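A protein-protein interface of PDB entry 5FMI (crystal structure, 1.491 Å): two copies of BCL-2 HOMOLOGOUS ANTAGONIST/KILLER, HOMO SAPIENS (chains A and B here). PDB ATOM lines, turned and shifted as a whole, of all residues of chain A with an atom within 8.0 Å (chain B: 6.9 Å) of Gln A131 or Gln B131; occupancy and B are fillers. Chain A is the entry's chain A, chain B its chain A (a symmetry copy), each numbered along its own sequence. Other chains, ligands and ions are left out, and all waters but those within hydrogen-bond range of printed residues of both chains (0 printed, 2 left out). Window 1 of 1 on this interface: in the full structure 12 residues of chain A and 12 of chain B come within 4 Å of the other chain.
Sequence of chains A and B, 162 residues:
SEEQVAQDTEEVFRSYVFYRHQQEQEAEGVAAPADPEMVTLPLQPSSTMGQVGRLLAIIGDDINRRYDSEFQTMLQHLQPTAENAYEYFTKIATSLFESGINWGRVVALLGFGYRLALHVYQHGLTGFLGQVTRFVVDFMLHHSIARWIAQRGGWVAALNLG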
ATOM      1  N   PHE A  13       3.609   7.396  10.387  1.00  0.00           N
ATOM      2  CA  PHE A  13       3.823   8.614  11.158  1.00  0.00           C
ATOM      3  C   PHE A  13       4.185   9.791  10.262  1.00  0.00           C
ATOM      4  O   PHE A  13       3.666  10.897  10.468  1.00  0.00           O
ATOM      5  CB  PHE A  13       4.890   8.403  12.238  1.00  0.00           C
ATOM      6  CG  PHE A  13       5.151   9.635  13.073  1.00  0.00           C
ATOM      7  CD1 PHE A  13       4.194  10.115  13.970  1.00  0.00           C
ATOM      8  CD2 PHE A  13       6.331  10.343  12.934  1.00  0.00           C
ATOM      9  CE1 PHE A  13       4.446  11.259  14.748  1.00  0.00           C
ATOM     10  CE2 PHE A  13       6.583  11.485  13.699  1.00  0.00           C
ATOM     11  CZ  PHE A  13       5.646  11.950  14.600  1.00  0.00           C
ATOM     12  N   ALA A  82      18.050  17.232  23.157  1.00  0.00           N
ATOM     13  CA  ALA A  82      17.562  15.945  22.665  1.00  0.00           C
ATOM     14  C   ALA A  82      17.262  14.991  23.815  1.00  0.00           C
ATOM     15  O   ALA A  82      16.311  14.195  23.742  1.00  0.00           O
ATOM     16  CB  ALA A  82      18.573  15.311  21.707  1.00  0.00           C
ATOM     17  N   GLU A  83      18.057  15.044  24.880  1.00  0.00           N
ATOM     18  CA  GLU A  83      17.783  14.201  26.031  1.00  0.00           C
ATOM     19  C   GLU A  83      16.476  14.597  26.696  1.00  0.00           C
ATOM     20  O   GLU A  83      15.674  13.730  27.064  1.00  0.00           O
ATOM     21  CB  GLU A  83      18.968  14.226  26.999  1.00  0.00           C
ATOM     22  CG  GLU A  83      18.806  13.287  28.162  1.00  0.00           C
ATOM     23  CD  GLU A  83      18.930  11.847  27.730  1.00  0.00           C
ATOM     24  OE1 GLU A  83      19.368  11.612  26.585  1.00  0.00           O
ATOM     25  OE2 GLU A  83      18.516  10.969  28.511  1.00  0.00           O
ATOM     26  N   ALA A  85      13.900  15.955  25.211  1.00  0.00           N
ATOM     27  CA  ALA A  85      12.824  15.498  24.334  1.00  0.00           C
ATOM     28  C   ALA A  85      12.565  14.004  24.500  1.00  0.00           C
ATOM     29  O   ALA A  85      11.403  13.571  24.552  1.00  0.00           O
ATOM     30  CB  ALA A  85      13.159  15.817  22.879  1.00  0.00           C
ATOM     31  N   TYR A  86      13.633  13.200  24.602  1.00  0.00           N
ATOM     32  CA  TYR A  86      13.465  11.764  24.786  1.00  0.00           C
ATOM     33  C   TYR A  86      12.802  11.455  26.122  1.00  0.00           C
ATOM     34  O   TYR A  86      11.901  10.610  26.200  1.00  0.00           O
ATOM     35  CB  TYR A  86      14.813  11.038  24.692  1.00  0.00           C
ATOM     36  CG  TYR A  86      14.665   9.570  25.056  1.00  0.00           C
ATOM     37  CD1 TYR A  86      14.115   8.673  24.143  1.00  0.00           C
ATOM     38  CD2 TYR A  86      15.034   9.096  26.319  1.00  0.00           C
ATOM     39  CE1 TYR A  86      13.947   7.336  24.470  1.00  0.00           C
ATOM     40  CE2 TYR A  86      14.862   7.757  26.656  1.00  0.00           C
ATOM     41  CZ  TYR A  86      14.319   6.893  25.720  1.00  0.00           C
ATOM     42  OH  TYR A  86      14.159   5.570  26.069  1.00  0.00           O
ATOM     43  N   GLU A  87      13.264  12.103  27.188  1.00  0.00           N
ATOM     44  CA  GLU A  87      12.715  11.829  28.511  1.00  0.00           C
ATOM     45  C   GLU A  87      11.244  12.210  28.578  1.00  0.00           C
ATOM     46  O   GLU A  87      10.417  11.450  29.102  1.00  0.00           O
ATOM     47  CB  GLU A  87      13.523  12.581  29.572  1.00  0.00           C
ATOM     48  CG  GLU A  87      14.954  12.065  29.749  1.00  0.00           C
ATOM     49  CD  GLU A  87      15.794  12.945  30.657  1.00  0.00           C
ATOM     50  OE1 GLU A  87      15.386  14.096  30.916  1.00  0.00           O
ATOM     51  OE2 GLU A  87      16.870  12.481  31.094  1.00  0.00           O
ATOM     52  N   PHE A  89       9.146  12.554  25.953  1.00  0.00           N
ATOM     53  CA  PHE A  89       8.440  11.622  25.082  1.00  0.00           C
ATOM     54  C   PHE A  89       8.146  10.307  25.797  1.00  0.00           C
ATOM     55  O   PHE A  89       7.023   9.790  25.737  1.00  0.00           O
ATOM     56  CB  PHE A  89       9.214  11.354  23.784  1.00  0.00           C
ATOM     57  CG  PHE A  89       8.591  10.272  22.952  1.00  0.00           C
ATOM     58  CD1 PHE A  89       8.933   8.938  23.150  1.00  0.00           C
ATOM     59  CD2 PHE A  89       7.619  10.575  22.016  1.00  0.00           C
ATOM     60  CE1 PHE A  89       8.319   7.930  22.426  1.00  0.00           C
ATOM     61  CE2 PHE A  89       7.011   9.573  21.281  1.00  0.00           C
ATOM     62  CZ  PHE A  89       7.351   8.257  21.489  1.00  0.00           C
ATOM     63  N   LEU A 116       5.170  17.215  19.708  1.00  0.00           N
ATOM     64  CA  LEU A 116       6.545  17.283  20.186  1.00  0.00           C
ATOM     65  C   LEU A 116       7.481  17.759  19.086  1.00  0.00           C
ATOM     66  O   LEU A 116       8.326  18.641  19.305  1.00  0.00           O
ATOM     67  CB  LEU A 116       6.966  15.919  20.726  1.00  0.00           C
ATOM     68  CG  LEU A 116       8.447  15.825  21.103  1.00  0.00           C
ATOM     69  CD1 LEU A 116       8.806  16.843  22.179  1.00  0.00           C
ATOM     70  CD2 LEU A 116       8.820  14.403  21.546  1.00  0.00           C
ATOM     71  N   ALA A 117       7.342  17.192  17.885  1.00  0.00           N
ATOM     72  CA  ALA A 117       8.190  17.602  16.769  1.00  0.00           C
ATOM     73  C   ALA A 117       8.010  19.081  16.448  1.00  0.00           C
ATOM     74  O   ALA A 117       8.993  19.804  16.237  1.00  0.00           O
ATOM     75  CB  ALA A 117       7.870  16.757  15.539  1.00  0.00           C
ATOM     76  N   VAL A 120       9.743  21.265  19.245  1.00  0.00           N
ATOM     77  CA  VAL A 120      11.200  21.337  19.260  1.00  0.00           C
ATOM     78  C   VAL A 120      11.704  22.152  18.075  1.00  0.00           C
ATOM     79  O   VAL A 120      12.692  22.887  18.201  1.00  0.00           O
ATOM     80  CB  VAL A 120      11.871  19.955  19.380  1.00  0.00           C
ATOM     81  CG1 VAL A 120      11.377  19.214  20.610  1.00  0.00           C
ATOM     82  CG2 VAL A 120      11.671  19.145  18.129  1.00  0.00           C
ATOM     83  N   LEU A 125      15.364  23.577  17.441  1.00  0.00           N
ATOM     84  CA  LEU A 125      15.956  22.269  17.184  1.00  0.00           C
ATOM     85  C   LEU A 125      15.481  21.812  15.806  1.00  0.00           C
ATOM     86  O   LEU A 125      14.388  21.249  15.668  1.00  0.00           O
ATOM     87  CB  LEU A 125      15.555  21.283  18.274  1.00  0.00           C
ATOM     88  CG  LEU A 125      16.407  20.019  18.410  1.00  0.00           C
ATOM     89  CD1 LEU A 125      17.879  20.372  18.501  1.00  0.00           C
ATOM     90  CD2 LEU A 125      15.961  19.216  19.633  1.00  0.00           C
ATOM     91  N   GLY A 127      16.061  19.602  12.131  1.00  0.00           N
ATOM     92  CA  GLY A 127      16.556  18.287  11.763  1.00  0.00           C
ATOM     93  C   GLY A 127      16.288  17.216  12.789  1.00  0.00           C
ATOM     94  O   GLY A 127      17.040  16.229  12.868  1.00  0.00           O
ATOM     95  N   PHE A 128      15.225  17.377  13.581  1.00  0.00           N
ATOM     96  CA  PHE A 128      14.877  16.459  14.651  1.00  0.00           C
ATOM     97  C   PHE A 128      13.599  15.684  14.351  1.00  0.00           C
ATOM     98  O   PHE A 128      13.203  14.833  15.154  1.00  0.00           O
ATOM     99  CB  PHE A 128      14.729  17.238  15.970  1.00  0.00           C
ATOM    100  CG  PHE A 128      14.986  16.412  17.193  1.00  0.00           C
ATOM    101  CD1 PHE A 128      16.280  16.090  17.547  1.00  0.00           C
ATOM    102  CD2 PHE A 128      13.941  15.951  17.982  1.00  0.00           C
ATOM    103  CE1 PHE A 128      16.528  15.323  18.666  1.00  0.00           C
ATOM    104  CE2 PHE A 128      14.192  15.177  19.106  1.00  0.00           C
ATOM    105  CZ  PHE A 128      15.484  14.868  19.443  1.00  0.00           C
ATOM    106  N   LEU A 129      12.962  15.924  13.198  1.00  0.00           N
ATOM    107  CA  LEU A 129      11.709  15.225  12.923  1.00  0.00           C
ATOM    108  C   LEU A 129      11.940  13.731  12.710  1.00  0.00           C
ATOM    109  O   LEU A 129      11.126  12.910  13.155  1.00  0.00           O
ATOM    110  CB  LEU A 129      10.986  15.867  11.734  1.00  0.00           C
ATOM    111  CG  LEU A 129       9.704  15.204  11.233  1.00  0.00           C
ATOM    112  CD1 LEU A 129       8.625  15.143  12.301  1.00  0.00           C
ATOM    113  CD2 LEU A 129       9.211  16.012  10.023  1.00  0.00           C
ATOM    114  N   GLY A 130      13.052  13.363  12.067  1.00  0.00           N
ATOM    115  CA  GLY A 130      13.391  11.949  11.962  1.00  0.00           C
ATOM    116  C   GLY A 130      13.620  11.306  13.319  1.00  0.00           C
ATOM    117  O   GLY A 130      13.230  10.154  13.546  1.00  0.00           O
ATOM    118  N   GLN A 131      14.217  12.055  14.256  1.00  0.00           N
ATOM    119  CA  GLN A 131      14.416  11.520  15.600  1.00  0.00           C
ATOM    120  C   GLN A 131      13.097  11.295  16.336  1.00  0.00           C
ATOM    121  O   GLN A 131      12.925  10.267  17.008  1.00  0.00           O
ATOM    122  CB  GLN A 131      15.349  12.420  16.410  1.00  0.00           C
ATOM    123  CG  GLN A 131      15.797  11.733  17.700  1.00  0.00           C
ATOM    124  CD  GLN A 131      16.496  10.414  17.411  1.00  0.00           C
ATOM    125  OE1 GLN A 131      17.526  10.377  16.721  1.00  0.00           O
ATOM    126  NE2 GLN A 131      15.924   9.315  17.913  1.00  0.00           N
ATOM    127  N   VAL A 132      12.146  12.229  16.222  1.00  0.00           N
ATOM    128  CA  VAL A 132      10.831  11.979  16.814  1.00  0.00           C
ATOM    129  C   VAL A 132      10.180  10.770  16.160  1.00  0.00           C
ATOM    130  O   VAL A 132       9.538   9.957  16.830  1.00  0.00           O
ATOM    131  CB  VAL A 132       9.920  13.218  16.713  1.00  0.00           C
ATOM    132  CG1 VAL A 132       8.534  12.904  17.283  1.00  0.00           C
ATOM    133  CG2 VAL A 132      10.538  14.417  17.437  1.00  0.00           C
ATOM    134  N   THR A 133      10.326  10.641  14.833  1.00  0.00           N
ATOM    135  CA  THR A 133       9.794   9.469  14.144  1.00  0.00           C
ATOM    136  C   THR A 133      10.372   8.193  14.735  1.00  0.00           C
ATOM    137  O   THR A 133       9.632   7.245  15.026  1.00  0.00           O
ATOM    138  CB  THR A 133      10.088   9.583  12.647  1.00  0.00           C
ATOM    139  OG1 THR A 133       9.505  10.796  12.136  1.00  0.00           O
ATOM    140  CG2 THR A 133       9.531   8.393  11.870  1.00  0.00           C
ATOM    141  N   ARG A 134      11.687   8.179  14.977  1.00  0.00           N
ATOM    142  CA  ARG A 134      12.312   7.011  15.585  1.00  0.00           C
ATOM    143  C   ARG A 134      11.826   6.785  17.010  1.00  0.00           C
ATOM    144  O   ARG A 134      11.657   5.635  17.427  1.00  0.00           O
ATOM    145  CB  ARG A 134      13.838   7.127  15.511  1.00  0.00           C
ATOM    146  CG  ARG A 134      14.381   7.051  14.095  1.00  0.00           C
ATOM    147  CD  ARG A 134      15.916   7.058  14.039  1.00  0.00           C
ATOM    148  NE  ARG A 134      16.506   8.353  14.376  1.00  0.00           N
ATOM    149  CZ  ARG A 134      16.627   9.365  13.515  1.00  0.00           C
ATOM    150  NH1 ARG A 134      16.179   9.224  12.272  1.00  0.00           N
ATOM    151  NH2 ARG A 134      17.190  10.507  13.895  1.00  0.00           N
ATOM    152  N   PHE A 135      11.611   7.855  17.782  1.00  0.00           N
ATOM    153  CA  PHE A 135      11.012   7.681  19.108  1.00  0.00           C
ATOM    154  C   PHE A 135       9.715   6.885  19.002  1.00  0.00           C
ATOM    155  O   PHE A 135       9.480   5.938  19.768  1.00  0.00           O
ATOM    156  CB  PHE A 135      10.691   9.032  19.760  1.00  0.00           C
ATOM    157  CG  PHE A 135      11.899   9.820  20.232  1.00  0.00           C
ATOM    158  CD1 PHE A 135      13.174   9.266  20.238  1.00  0.00           C
ATOM    159  CD2 PHE A 135      11.729  11.118  20.687  1.00  0.00           C
ATOM    160  CE1 PHE A 135      14.271  10.010  20.670  1.00  0.00           C
ATOM    161  CE2 PHE A 135      12.838  11.862  21.127  1.00  0.00           C
ATOM    162  CZ  PHE A 135      14.089  11.301  21.120  1.00  0.00           C
ATOM    163  N   VAL A 136       8.860   7.269  18.050  1.00  0.00           N
ATOM    164  CA  VAL A 136       7.549   6.643  17.911  1.00  0.00           C
ATOM    165  C   VAL A 136       7.688   5.197  17.456  1.00  0.00           C
ATOM    166  O   VAL A 136       7.073   4.290  18.030  1.00  0.00           O
ATOM    167  CB  VAL A 136       6.680   7.457  16.935  1.00  0.00           C
ATOM    168  CG1 VAL A 136       5.388   6.706  16.621  1.00  0.00           C
ATOM    169  CG2 VAL A 136       6.377   8.820  17.503  1.00  0.00           C
ATOM    170  N   VAL A 137       8.475   4.971  16.401  1.00  0.00           N
ATOM    171  CA  VAL A 137       8.666   3.630  15.850  1.00  0.00           C
ATOM    172  C   VAL A 137       9.187   2.697  16.925  1.00  0.00           C
ATOM    173  O   VAL A 137       8.655   1.600  17.145  1.00  0.00           O
ATOM    174  CB  VAL A 137       9.649   3.694  14.667  1.00  0.00           C
ATOM    175  CG1 VAL A 137      10.065   2.285  14.238  1.00  0.00           C
ATOM    176  CG2 VAL A 137       9.032   4.461  13.503  1.00  0.00           C
ATOM    177  N   ASP A 138      10.249   3.120  17.611  1.00  0.00           N
ATOM    178  CA  ASP A 138      10.903   2.236  18.564  1.00  0.00           C
ATOM    179  C   ASP A 138      10.042   2.013  19.801  1.00  0.00           C
ATOM    180  O   ASP A 138      10.007   0.903  20.344  1.00  0.00           O
ATOM    181  CB  ASP A 138      12.273   2.791  18.941  1.00  0.00           C
ATOM    182  CG  ASP A 138      13.257   1.698  19.337  1.00  0.00           C
ATOM    183  OD1 ASP A 138      13.379   0.679  18.608  1.00  0.00           O
ATOM    184  OD2 ASP A 138      13.896   1.846  20.399  1.00  0.00           O
ATOM    185  N   ALA B  82      20.664  16.285  14.241  1.00  0.00           N
ATOM    186  CA  ALA B  82      20.445  14.954  14.804  1.00  0.00           C
ATOM    187  C   ALA B  82      20.209  13.922  13.707  1.00  0.00           C
ATOM    188  O   ALA B  82      20.631  12.760  13.833  1.00  0.00           O
ATOM    189  CB  ALA B  82      19.266  14.964  15.779  1.00  0.00           C
ATOM    190  N   GLU B  83      19.534  14.314  12.630  1.00  0.00           N
ATOM    191  CA  GLU B  83      19.331  13.391  11.527  1.00  0.00           C
ATOM    192  C   GLU B  83      20.651  13.042  10.861  1.00  0.00           C
ATOM    193  O   GLU B  83      20.903  11.872  10.548  1.00  0.00           O
ATOM    194  CB  GLU B  83      18.307  13.961  10.543  1.00  0.00           C
ATOM    195  CG  GLU B  83      17.958  13.010   9.430  1.00  0.00           C
ATOM    196  CD  GLU B  83      17.132  11.852   9.933  1.00  0.00           C
ATOM    197  OE1 GLU B  83      16.652  11.928  11.083  1.00  0.00           O
ATOM    198  OE2 GLU B  83      17.038  10.848   9.203  1.00  0.00           O
ATOM    199  N   TYR B  86      22.432  10.512  13.061  1.00  0.00           N
ATOM    200  CA  TYR B  86      21.853   9.179  12.951  1.00  0.00           C
ATOM    201  C   TYR B  86      22.252   8.511  11.642  1.00  0.00           C
ATOM    202  O   TYR B  86      22.604   7.325  11.618  1.00  0.00           O
ATOM    203  CB  TYR B  86      20.324   9.235  13.063  1.00  0.00           C
ATOM    204  CG  TYR B  86      19.708   7.877  12.776  1.00  0.00           C
ATOM    205  CD1 TYR B  86      19.744   6.871  13.740  1.00  0.00           C
ATOM    206  CD2 TYR B  86      19.133   7.589  11.533  1.00  0.00           C
ATOM    207  CE1 TYR B  86      19.213   5.617  13.483  1.00  0.00           C
ATOM    208  CE2 TYR B  86      18.604   6.331  11.266  1.00  0.00           C
ATOM    209  CZ  TYR B  86      18.650   5.360  12.252  1.00  0.00           C
ATOM    210  OH  TYR B  86      18.118   4.120  11.972  1.00  0.00           O
ATOM    211  N   GLY B 127      23.725  17.883  25.160  1.00  0.00           N
ATOM    212  CA  GLY B 127      22.641  17.016  25.587  1.00  0.00           C
ATOM    213  C   GLY B 127      22.320  15.906  24.620  1.00  0.00           C
ATOM    214  O   GLY B 127      21.172  15.428  24.580  1.00  0.00           O
ATOM    215  N   PHE B 128      23.309  15.470  23.835  1.00  0.00           N
ATOM    216  CA  PHE B 128      23.133  14.449  22.818  1.00  0.00           C
ATOM    217  C   PHE B 128      23.851  13.153  23.174  1.00  0.00           C
ATOM    218  O   PHE B 128      23.754  12.178  22.420  1.00  0.00           O
ATOM    219  CB  PHE B 128      23.635  14.980  21.463  1.00  0.00           C
ATOM    220  CG  PHE B 128      22.980  14.336  20.279  1.00  0.00           C
ATOM    221  CD1 PHE B 128      21.696  14.691  19.925  1.00  0.00           C
ATOM    222  CD2 PHE B 128      23.641  13.372  19.529  1.00  0.00           C
ATOM    223  CE1 PHE B 128      21.080  14.098  18.843  1.00  0.00           C
ATOM    224  CE2 PHE B 128      23.019  12.774  18.442  1.00  0.00           C
ATOM    225  CZ  PHE B 128      21.743  13.141  18.104  1.00  0.00           C
ATOM    226  N   LEU B 129      24.538  13.096  24.322  1.00  0.00           N
ATOM    227  CA  LEU B 129      25.272  11.877  24.648  1.00  0.00           C
ATOM    228  C   LEU B 129      24.324  10.715  24.933  1.00  0.00           C
ATOM    229  O   LEU B 129      24.608   9.575  24.541  1.00  0.00           O
ATOM    230  CB  LEU B 129      26.236  12.127  25.813  1.00  0.00           C
ATOM    231  CG  LEU B 129      27.018  10.935  26.364  1.00  0.00           C
ATOM    232  CD1 LEU B 129      27.904  10.285  25.315  1.00  0.00           C
ATOM    233  CD2 LEU B 129      27.866  11.445  27.539  1.00  0.00           C
ATOM    234  N   GLY B 130      23.187  10.990  25.578  1.00  0.00           N
ATOM    235  CA  GLY B 130      22.183   9.945  25.750  1.00  0.00           C
ATOM    236  C   GLY B 130      21.644   9.438  24.423  1.00  0.00           C
ATOM    237  O   GLY B 130      21.399   8.237  24.260  1.00  0.00           O
ATOM    238  N   GLN B 131      21.493  10.337  23.442  1.00  0.00           N
ATOM    239  CA  GLN B 131      21.033   9.909  22.124  1.00  0.00           C
ATOM    240  C   GLN B 131      22.049   9.013  21.419  1.00  0.00           C
ATOM    241  O   GLN B 131      21.671   8.006  20.802  1.00  0.00           O
ATOM    242  CB  GLN B 131      20.668  11.114  21.257  1.00  0.00           C
ATOM    243  CG  GLN B 131      19.918  10.682  19.998  1.00  0.00           C
ATOM    244  CD  GLN B 131      18.654   9.911  20.343  1.00  0.00           C
ATOM    245  OE1 GLN B 131      17.755  10.431  21.020  1.00  0.00           O
ATOM    246  NE2 GLN B 131      18.589   8.649  19.904  1.00  0.00           N
ATOM    247  N   VAL B 132      23.342   9.347  21.498  1.00  0.00           N
ATOM    248  CA  VAL B 132      24.345   8.439  20.938  1.00  0.00           C
ATOM    249  C   VAL B 132      24.308   7.102  21.660  1.00  0.00           C
ATOM    250  O   VAL B 132      24.444   6.043  21.041  1.00  0.00           O
ATOM    251  CB  VAL B 132      25.757   9.055  20.988  1.00  0.00           C
ATOM    252  CG1 VAL B 132      26.789   8.058  20.454  1.00  0.00           C
ATOM    253  CG2 VAL B 132      25.816  10.364  20.197  1.00  0.00           C
ATOM    254  N   THR B 133      24.135   7.130  22.990  1.00  0.00           N
ATOM    255  CA  THR B 133      24.014   5.886  23.744  1.00  0.00           C
ATOM    256  C   THR B 133      22.865   5.046  23.210  1.00  0.00           C
ATOM    257  O   THR B 133      23.022   3.842  22.977  1.00  0.00           O
ATOM    258  CB  THR B 133      23.838   6.208  25.230  1.00  0.00           C
ATOM    259  OG1 THR B 133      24.959   6.987  25.687  1.00  0.00           O
ATOM    260  CG2 THR B 133      23.731   4.939  26.072  1.00  0.00           C
ATOM    261  N   ARG B 134      21.718   5.684  22.951  1.00  0.00           N
ATOM    262  CA  ARG B 134      20.581   4.961  22.395  1.00  0.00           C
ATOM    263  C   ARG B 134      20.869   4.449  20.990  1.00  0.00           C
ATOM    264  O   ARG B 134      20.430   3.351  20.633  1.00  0.00           O
ATOM    265  CB  ARG B 134      19.323   5.832  22.441  1.00  0.00           C
ATOM    266  CG  ARG B 134      18.834   6.111  23.852  1.00  0.00           C
ATOM    267  CD  ARG B 134      17.513   6.892  23.887  1.00  0.00           C
ATOM    268  NE  ARG B 134      17.650   8.289  23.478  1.00  0.00           N
ATOM    269  CZ  ARG B 134      18.067   9.267  24.285  1.00  0.00           C
ATOM    270  NH1 ARG B 134      18.399   8.982  25.539  1.00  0.00           N
ATOM    271  NH2 ARG B 134      18.149  10.516  23.840  1.00  0.00           N
ATOM    272  N   PHE B 135      21.583   5.226  20.167  1.00  0.00           N
ATOM    273  CA  PHE B 135      21.995   4.707  18.861  1.00  0.00           C
ATOM    274  C   PHE B 135      22.716   3.373  19.024  1.00  0.00           C
ATOM    275  O   PHE B 135      22.432   2.399  18.309  1.00  0.00           O
ATOM    276  CB  PHE B 135      22.943   5.678  18.145  1.00  0.00           C
ATOM    277  CG  PHE B 135      22.289   6.942  17.618  1.00  0.00           C
ATOM    278  CD1 PHE B 135      20.909   7.106  17.623  1.00  0.00           C
ATOM    279  CD2 PHE B 135      23.083   7.954  17.101  1.00  0.00           C
ATOM    280  CE1 PHE B 135      20.329   8.278  17.139  1.00  0.00           C
ATOM    281  CE2 PHE B 135      22.493   9.131  16.609  1.00  0.00           C
ATOM    282  CZ  PHE B 135      21.130   9.277  16.627  1.00  0.00           C
ATOM    283  N   VAL B 136      23.661   3.322  19.966  1.00  0.00           N
ATOM    284  CA  VAL B 136      24.480   2.129  20.154  1.00  0.00           C
ATOM    285  C   VAL B 136      23.639   0.974  20.680  1.00  0.00           C
ATOM    286  O   VAL B 136      23.706  -0.146  20.160  1.00  0.00           O
ATOM    287  CB  VAL B 136      25.654   2.443  21.100  1.00  0.00           C
ATOM    288  CG1 VAL B 136      26.397   1.160  21.469  1.00  0.00           C
ATOM    289  CG2 VAL B 136      26.594   3.439  20.468  1.00  0.00           C
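Glu A83 touches Arg B134, and with the chains exchanged Arg A134 touches Glu B83. Tyr A86 touches Arg B134, and with the chains exchanged Arg A134 touches Tyr B86. Gln B131 touches its own counterpart, Gln A131. Gln A131 touches Phe B135, and with the chains exchanged Phe A135 touches Gln B131. Positions printed for both chains: 82, 83, 86, 127, 128, 129, 130, 131, 132, 133, 134, 135 and 136.
The backbone carbonyl oxygen (O) of Gly A127 lies within hydrogen-bond range of the backbone NH (N) of Glu B83, 3.2 Å away. The guanidinium group (NH1) of Arg A134 lies within salt-bridge range of the side-chain carboxylate (OE1) of Glu B83 (3.0 Å). OE1 of Glu A83 is in salt-bridge range of NH1 of Arg B134 (3.0 Å). The side-chain amide nitrogen (NE2) of Gln B131 lies close to the side-chain amide nitrogen (NE2) of Gln A131 (3.4 Å). N of Glu A83 sits at hydrogen-bond distance from O of Gly B127, at 3.2 Å.
Glu A87 touches none of the printed residues of chain B. Ala A117 touches none of the printed residues of chain B. Printed residues of chain B within 4 Å of Gly A127: Ala B82 (3.9 Å) and Glu B83 (3.2 Å). Printed residues of chain B within 4 Å of Gly A130: Glu B83 (3.4 Å). Printed residues of chain B within 4 Å of Gln A131: Gln B131 (3.4 Å) and Phe B135 (3.5 Å). Printed residues of chain A within 4 Å of Gly B130: Glu A83. Of the printed residues of chain A, Gln B131 touches Gln A131 and Phe A135. Printed residues of chain A within 4 Å of Arg B134: Glu A83 (3.0 Å) and Tyr A86 (3.5 Å). The nearest printed residue of chain A that does not touch Gln B131 is Glu A83 (4.002 Å).
The backbone carbonyl oxygen (O) of Gly A130 lies within hydrogen-bond range of the guanidinium group (NH1) of Arg A134, 3.3 Å away. The side-chain amide oxygen (OE1) of Gln A131 sits at hydrogen-bond distance from the guanidinium group (NH2) of Arg A134 (2.8 Å). The side-chain amide oxygen of Gln B131 sits at hydrogen-bond distance from the guanidinium group of Arg B134, at 2.8 Å. O of Gly B130 lies within hydrogen-bond range of NH1 of Arg B134, at 3.3 Å.
Hydrophobic or aromatic side chains of chain A within 4 Å of the printed part of chain B: Ala A82, Tyr A86, Phe A128 and Phe A135. Printed residues of chain B that touch a printed residue of chain A: Ala B82, Glu B83, Tyr B86, Gly B127, Phe B128, Gly B130, Gln B131, Arg B134 and Phe B135. Hydrophobic or aromatic side chains of chain B within 4 Å of the printed part of chain A: Ala B82, Tyr B86, Phe B128 and Phe B135. Among the printed residues, 15 pairs touch across the chains.
Among the printed residues, pairs that only touch across the chains: Glu A83 with Gly B130 (3.4 Å), Gly A130 with Glu B83 (3.4 Å), Tyr A86 with Arg B134 (3.5 Å), Arg A134 with Tyr B86 (3.5 Å), Gln A131 with Phe B135 (3.5 Å), Phe A135 with Gln B131 (3.5 Å), Phe A128 with Ala B82 (3.6 Å), Ala A82 with Phe B128 (3.6 Å), Gly A127 with Ala B82 (3.9 Å) and Ala A82 with Gly B127 (3.9 Å).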
